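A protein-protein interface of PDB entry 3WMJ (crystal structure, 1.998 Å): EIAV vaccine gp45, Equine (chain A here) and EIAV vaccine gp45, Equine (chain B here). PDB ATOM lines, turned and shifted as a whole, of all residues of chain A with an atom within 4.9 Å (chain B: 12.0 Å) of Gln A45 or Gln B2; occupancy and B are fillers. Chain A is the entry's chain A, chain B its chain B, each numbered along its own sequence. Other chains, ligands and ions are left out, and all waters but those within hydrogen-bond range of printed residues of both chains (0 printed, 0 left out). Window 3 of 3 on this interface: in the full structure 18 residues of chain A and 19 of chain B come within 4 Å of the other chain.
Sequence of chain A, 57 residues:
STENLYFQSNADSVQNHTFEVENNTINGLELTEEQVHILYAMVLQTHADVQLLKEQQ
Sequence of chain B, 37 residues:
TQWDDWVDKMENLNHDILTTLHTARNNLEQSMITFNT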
ATOM      1  N   ALA A  41      -6.683 -10.768   0.779  1.00  0.00           N
ATOM      2  CA  ALA A  41      -6.607  -9.333   0.513  1.00  0.00           C
ATOM      3  C   ALA A  41      -7.169  -8.971  -0.862  1.00  0.00           C
ATOM      4  O   ALA A  41      -7.966  -8.026  -0.985  1.00  0.00           O
ATOM      5  CB  ALA A  41      -5.183  -8.856   0.634  1.00  0.00           C
ATOM      6  N   MET A  42      -6.745  -9.702  -1.899  1.00  0.00           N
ATOM      7  CA  MET A  42      -7.233  -9.453  -3.257  1.00  0.00           C
ATOM      8  C   MET A  42      -8.756  -9.589  -3.339  1.00  0.00           C
ATOM      9  O   MET A  42      -9.426  -8.780  -3.991  1.00  0.00           O
ATOM     10  CB  MET A  42      -6.556 -10.394  -4.268  1.00  0.00           C
ATOM     11  CG  MET A  42      -5.028 -10.278  -4.275  1.00  0.00           C
ATOM     12  SD  MET A  42      -4.188 -11.578  -5.206  1.00  0.00           S
ATOM     13  CE  MET A  42      -4.026 -10.796  -6.815  1.00  0.00           C
ATOM     14  N   VAL A  43      -9.285 -10.611  -2.672  1.00  0.00           N
ATOM     15  CA  VAL A  43     -10.714 -10.897  -2.655  1.00  0.00           C
ATOM     16  C   VAL A  43     -11.500  -9.789  -1.946  1.00  0.00           C
ATOM     17  O   VAL A  43     -12.570  -9.385  -2.411  1.00  0.00           O
ATOM     18  CB  VAL A  43     -10.989 -12.258  -1.964  1.00  0.00           C
ATOM     19  CG1 VAL A  43     -12.469 -12.406  -1.615  1.00  0.00           C
ATOM     20  CG2 VAL A  43     -10.540 -13.408  -2.848  1.00  0.00           C
ATOM     21  N   LEU A  44     -10.981  -9.310  -0.817  1.00  0.00           N
ATOM     22  CA  LEU A  44     -11.629  -8.223  -0.090  1.00  0.00           C
ATOM     23  C   LEU A  44     -11.638  -6.952  -0.940  1.00  0.00           C
ATOM     24  O   LEU A  44     -12.627  -6.229  -0.975  1.00  0.00           O
ATOM     25  CB  LEU A  44     -10.922  -7.953   1.242  1.00  0.00           C
ATOM     26  CG  LEU A  44     -11.129  -8.958   2.370  1.00  0.00           C
ATOM     27  CD1 LEU A  44     -10.294  -8.562   3.589  1.00  0.00           C
ATOM     28  CD2 LEU A  44     -12.597  -9.075   2.737  1.00  0.00           C
ATOM     29  N   GLN A  45     -10.536  -6.685  -1.626  1.00  0.00           N
ATOM     30  CA  GLN A  45     -10.421  -5.472  -2.431  1.00  0.00           C
ATOM     31  C   GLN A  45     -11.388  -5.508  -3.608  1.00  0.00           C
ATOM     32  O   GLN A  45     -12.036  -4.499  -3.921  1.00  0.00           O
ATOM     33  CB  GLN A  45      -8.984  -5.297  -2.923  1.00  0.00           C
ATOM     34  CG  GLN A  45      -8.823  -4.197  -3.975  1.00  0.00           C
ATOM     35  CD  GLN A  45      -8.974  -2.813  -3.382  1.00  0.00           C
ATOM     36  OE1 GLN A  45      -8.457  -2.534  -2.294  1.00  0.00           O
ATOM     37  NE2 GLN A  45      -9.684  -1.933  -4.091  1.00  0.00           N
ATOM     38  N   THR A  46     -11.499  -6.678  -4.235  1.00  0.00           N
ATOM     39  CA  THR A  46     -12.416  -6.869  -5.358  1.00  0.00           C
ATOM     40  C   THR A  46     -13.864  -6.729  -4.908  1.00  0.00           C
ATOM     41  O   THR A  46     -14.694  -6.158  -5.621  1.00  0.00           O
ATOM     42  CB  THR A  46     -12.208  -8.240  -6.024  1.00  0.00           C
ATOM     43  OG1 THR A  46     -10.845  -8.352  -6.454  1.00  0.00           O
ATOM     44  CG2 THR A  46     -13.121  -8.394  -7.240  1.00  0.00           C
ATOM     45  N   HIS A  47     -14.165  -7.251  -3.725  1.00  0.00           N
ATOM     46  CA  HIS A  47     -15.499  -7.099  -3.146  1.00  0.00           C
ATOM     47  C   HIS A  47     -15.850  -5.622  -2.957  1.00  0.00           C
ATOM     48  O   HIS A  47     -16.966  -5.199  -3.257  1.00  0.00           O
ATOM     49  CB  HIS A  47     -15.572  -7.832  -1.801  1.00  0.00           C
ATOM     50  CG  HIS A  47     -16.899  -7.718  -1.109  1.00  0.00           C
ATOM     51  ND1 HIS A  47     -18.036  -8.339  -1.575  1.00  0.00           N
ATOM     52  CD2 HIS A  47     -17.259  -7.078   0.030  1.00  0.00           C
ATOM     53  CE1 HIS A  47     -19.046  -8.075  -0.764  1.00  0.00           C
ATOM     54  NE2 HIS A  47     -18.601  -7.307   0.219  1.00  0.00           N
ATOM     55  N   ALA A  48     -14.905  -4.839  -2.443  1.00  0.00           N
ATOM     56  CA  ALA A  48     -15.133  -3.403  -2.270  1.00  0.00           C
ATOM     57  C   ALA A  48     -15.396  -2.736  -3.620  1.00  0.00           C
ATOM     58  O   ALA A  48     -16.280  -1.867  -3.733  1.00  0.00           O
ATOM     59  CB  ALA A  48     -13.945  -2.756  -1.576  1.00  0.00           C
ATOM     60  N   ASP A  49     -14.623  -3.112  -4.640  1.00  0.00           N
ATOM     61  CA  ASP A  49     -14.847  -2.546  -5.975  1.00  0.00           C
ATOM     62  C   ASP A  49     -16.233  -2.903  -6.497  1.00  0.00           C
ATOM     63  O   ASP A  49     -16.925  -2.070  -7.104  1.00  0.00           O
ATOM     64  CB  ASP A  49     -13.786  -3.021  -6.978  1.00  0.00           C
ATOM     65  CG  ASP A  49     -12.387  -2.482  -6.668  1.00  0.00           C
ATOM     66  OD1 ASP A  49     -12.271  -1.430  -5.989  1.00  0.00           O
ATOM     67  OD2 ASP A  49     -11.398  -3.120  -7.115  1.00  0.00           O
ATOM     68  N   THR B   1       1.297  -0.292  -8.284  1.00  0.00           N
ATOM     69  CA  THR B   1      -0.009  -0.405  -7.646  1.00  0.00           C
ATOM     70  C   THR B   1      -0.004  -1.516  -6.606  1.00  0.00           C
ATOM     71  O   THR B   1       0.816  -2.443  -6.662  1.00  0.00           O
ATOM     72  CB  THR B   1      -1.127  -0.756  -8.651  1.00  0.00           C
ATOM     73  OG1 THR B   1      -0.839  -2.027  -9.260  1.00  0.00           O
ATOM     74  CG2 THR B   1      -1.283   0.325  -9.721  1.00  0.00           C
ATOM     75  N   GLN B   2      -0.938  -1.425  -5.669  1.00  0.00           N
ATOM     76  CA  GLN B   2      -1.109  -2.462  -4.670  1.00  0.00           C
ATOM     77  C   GLN B   2      -1.403  -3.809  -5.345  1.00  0.00           C
ATOM     78  O   GLN B   2      -0.878  -4.841  -4.918  1.00  0.00           O
ATOM     79  CB  GLN B   2      -2.197  -2.058  -3.671  1.00  0.00           C
ATOM     80  CG  GLN B   2      -3.288  -3.084  -3.464  1.00  0.00           C
ATOM     81  CD  GLN B   2      -4.437  -2.552  -2.627  1.00  0.00           C
ATOM     82  OE1 GLN B   2      -5.503  -2.220  -3.156  1.00  0.00           O
ATOM     83  NE2 GLN B   2      -4.235  -2.486  -1.310  1.00  0.00           N
ATOM     84  N   TRP B   3      -2.207  -3.810  -6.406  1.00  0.00           N
ATOM     85  CA  TRP B   3      -2.525  -5.068  -7.084  1.00  0.00           C
ATOM     86  C   TRP B   3      -1.275  -5.710  -7.710  1.00  0.00           C
ATOM     87  O   TRP B   3      -1.072  -6.933  -7.604  1.00  0.00           O
ATOM     88  CB  TRP B   3      -3.610  -4.868  -8.144  1.00  0.00           C
ATOM     89  CG  TRP B   3      -4.192  -6.163  -8.622  1.00  0.00           C
ATOM     90  CD1 TRP B   3      -3.794  -6.899  -9.700  1.00  0.00           C
ATOM     91  CD2 TRP B   3      -5.281  -6.879  -8.024  1.00  0.00           C
ATOM     92  NE1 TRP B   3      -4.567  -8.040  -9.807  1.00  0.00           N
ATOM     93  CE2 TRP B   3      -5.493  -8.045  -8.793  1.00  0.00           C
ATOM     94  CE3 TRP B   3      -6.104  -6.635  -6.925  1.00  0.00           C
ATOM     95  CZ2 TRP B   3      -6.492  -8.977  -8.484  1.00  0.00           C
ATOM     96  CZ3 TRP B   3      -7.103  -7.554  -6.620  1.00  0.00           C
ATOM     97  CH2 TRP B   3      -7.289  -8.711  -7.396  1.00  0.00           C
ATOM     98  N   ASP B   4      -0.439  -4.898  -8.356  1.00  0.00           N
ATOM     99  CA  ASP B   4       0.798  -5.408  -8.963  1.00  0.00           C
ATOM    100  C   ASP B   4       1.756  -6.011  -7.927  1.00  0.00           C
ATOM    101  O   ASP B   4       2.481  -6.984  -8.217  1.00  0.00           O
ATOM    102  CB  ASP B   4       1.523  -4.300  -9.735  1.00  0.00           C
ATOM    103  CG  ASP B   4       0.835  -3.933 -11.037  1.00  0.00           C
ATOM    104  OD1 ASP B   4       0.107  -4.775 -11.608  1.00  0.00           O
ATOM    105  OD2 ASP B   4       1.043  -2.789 -11.498  1.00  0.00           O
ATOM    106  N   ASP B   5       1.771  -5.439  -6.725  1.00  0.00           N
ATOM    107  CA  ASP B   5       2.682  -5.919  -5.683  1.00  0.00           C
ATOM    108  C   ASP B   5       2.203  -7.259  -5.130  1.00  0.00           C
ATOM    109  O   ASP B   5       3.012  -8.123  -4.826  1.00  0.00           O
ATOM    110  CB  ASP B   5       2.828  -4.900  -4.546  1.00  0.00           C
ATOM    111  CG  ASP B   5       3.694  -3.699  -4.930  1.00  0.00           C
ATOM    112  OD1 ASP B   5       4.397  -3.755  -5.972  1.00  0.00           O
ATOM    113  OD2 ASP B   5       3.681  -2.705  -4.167  1.00  0.00           O
ATOM    114  N   TRP B   6       0.885  -7.413  -5.000  1.00  0.00           N
ATOM    115  CA  TRP B   6       0.290  -8.696  -4.600  1.00  0.00           C
ATOM    116  C   TRP B   6       0.652  -9.761  -5.604  1.00  0.00           C
ATOM    117  O   TRP B   6       1.061 -10.863  -5.233  1.00  0.00           O
ATOM    118  CB  TRP B   6      -1.236  -8.584  -4.533  1.00  0.00           C
ATOM    119  CG  TRP B   6      -1.722  -7.892  -3.309  1.00  0.00           C
ATOM    120  CD1 TRP B   6      -1.072  -7.793  -2.105  1.00  0.00           C
ATOM    121  CD2 TRP B   6      -2.964  -7.195  -3.152  1.00  0.00           C
ATOM    122  NE1 TRP B   6      -1.843  -7.082  -1.213  1.00  0.00           N
ATOM    123  CE2 TRP B   6      -3.006  -6.703  -1.833  1.00  0.00           C
ATOM    124  CE3 TRP B   6      -4.048  -6.942  -4.009  1.00  0.00           C
ATOM    125  CZ2 TRP B   6      -4.093  -5.961  -1.345  1.00  0.00           C
ATOM    126  CZ3 TRP B   6      -5.121  -6.212  -3.523  1.00  0.00           C
ATOM    127  CH2 TRP B   6      -5.139  -5.739  -2.199  1.00  0.00           C
ATOM    128  N   VAL B   7       0.488  -9.434  -6.882  1.00  0.00           N
ATOM    129  CA  VAL B   7       0.839 -10.343  -7.965  1.00  0.00           C
ATOM    130  C   VAL B   7       2.300 -10.764  -7.882  1.00  0.00           C
ATOM    131  O   VAL B   7       2.616 -11.956  -7.991  1.00  0.00           O
ATOM    132  CB  VAL B   7       0.553  -9.716  -9.335  1.00  0.00           C
ATOM    133  CG1 VAL B   7       1.228 -10.519 -10.429  1.00  0.00           C
ATOM    134  CG2 VAL B   7      -0.954  -9.651  -9.568  1.00  0.00           C
ATOM    135  N   ASP B   8       3.190  -9.798  -7.667  1.00  0.00           N
ATOM    136  CA  ASP B   8       4.615 -10.107  -7.582  1.00  0.00           C
ATOM    137  C   ASP B   8       4.946 -11.003  -6.371  1.00  0.00           C
ATOM    138  O   ASP B   8       5.786 -11.902  -6.471  1.00  0.00           O
ATOM    139  CB  ASP B   8       5.443  -8.820  -7.537  1.00  0.00           C
ATOM    140  CG  ASP B   8       5.499  -8.108  -8.883  1.00  0.00           C
ATOM    141  OD1 ASP B   8       5.026  -8.674  -9.898  1.00  0.00           O
ATOM    142  OD2 ASP B   8       6.030  -6.977  -8.921  1.00  0.00           O
ATOM    143  N   LYS B   9       4.285 -10.742  -5.242  1.00  0.00           N
ATOM    144  CA  LYS B   9       4.428 -11.558  -4.033  1.00  0.00           C
ATOM    145  C   LYS B   9       3.915 -12.971  -4.276  1.00  0.00           C
ATOM    146  O   LYS B   9       4.544 -13.949  -3.885  1.00  0.00           O
ATOM    147  CB  LYS B   9       3.643 -10.935  -2.870  1.00  0.00           C
ATOM    148  CG  LYS B   9       4.312  -9.728  -2.213  1.00  0.00           C
ATOM    149  CD  LYS B   9       3.635  -9.402  -0.879  1.00  0.00           C
ATOM    150  CE  LYS B   9       4.432  -8.391  -0.055  1.00  0.00           C
ATOM    151  NZ  LYS B   9       3.998  -6.987  -0.283  1.00  0.00           N
ATOM    152  N   MET B  10       2.758 -13.078  -4.922  1.00  0.00           N
ATOM    153  CA  MET B  10       2.184 -14.386  -5.224  1.00  0.00           C
ATOM    154  C   MET B  10       3.148 -15.226  -6.082  1.00  0.00           C
ATOM    155  O   MET B  10       3.354 -16.417  -5.810  1.00  0.00           O
ATOM    156  CB  MET B  10       0.814 -14.225  -5.908  1.00  0.00           C
ATOM    157  CG  MET B  10       0.062 -15.531  -6.144  1.00  0.00           C
ATOM    158  SD  MET B  10      -0.318 -16.496  -4.652  1.00  0.00           S
ATOM    159  CE  MET B  10      -1.368 -15.371  -3.771  1.00  0.00           C
ATOM    160  N   GLU B  11       3.754 -14.604  -7.096  1.00  0.00           N
ATOM    161  CA  GLU B  11       4.671 -15.321  -7.983  1.00  0.00           C
ATOM    162  C   GLU B  11       5.896 -15.827  -7.225  1.00  0.00           C
ATOM    163  O   GLU B  11       6.348 -16.964  -7.423  1.00  0.00           O
ATOM    164  CB  GLU B  11       5.127 -14.448  -9.169  1.00  0.00           C
ATOM    165  CG  GLU B  11       4.024 -13.727  -9.950  1.00  0.00           C
ATOM    166  CD  GLU B  11       2.955 -14.645 -10.538  1.00  0.00           C
ATOM    167  OE1 GLU B  11       3.270 -15.791 -10.930  1.00  0.00           O
ATOM    168  OE2 GLU B  11       1.785 -14.202 -10.626  1.00  0.00           O
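CB of Ala A41 touches CZ2 of Trp B6, at 3.7 Å.
Met A42 touches Trp B3.
Met A42 touches Trp B6 (CG to CE3, 3.5 Å).
Trp B6 touches Gln A45 (CH2 to CB, 3.9 Å).
Thr A46 touches Trp B3.
OG1 of Thr A46 is in hydrogen-bond range of O of Met A42 (2.9 Å).
OD1 of Asp A49 sits at hydrogen-bond distance from NE2 of Gln A45.
The side-chain amide oxygen (OE1) of Gln A45 lies close to the side-chain amide oxygen (OE1) of Gln B2, at 3.1 Å.
Hydrophobic or aromatic side chains of chain A within 4 Å of the printed part of chain B: Ala A41 and Met A42.
Of the 11 printed residues of chain B, 3 touch a printed residue of chain A.
Hydrophobic or aromatic side chains of chain B within 4 Å of the printed part of chain A: Trp B3 and Trp B6.
Gln B2 touches just one residue of chain A: Gln A45 (3.1 Å).
Ala A41 touches one residue of chain B.
Met A42 touches two residues of chain B.
No residue of chain B comes within 4 Å of Leu A44.
No residue of chain B comes within 4 Å of Ala A48.
No residue of chain B comes within 4 Å of Asp A49.
Printed residues of chain A within 4 Å of Trp B6: Ala A41 (3.7 Å), Met A42 (3.5 Å) and Gln A45 (3.9 Å).
Of the printed residues of chain A, Trp B3 touches Met A42 and Thr A46.
Lys B9 touches none of the printed residues of chain A.
Val B7 touches none of the printed residues of chain A.
The nearest residue of chain B that does not touch Gln A45 is Trp B3 (4.6 Å).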
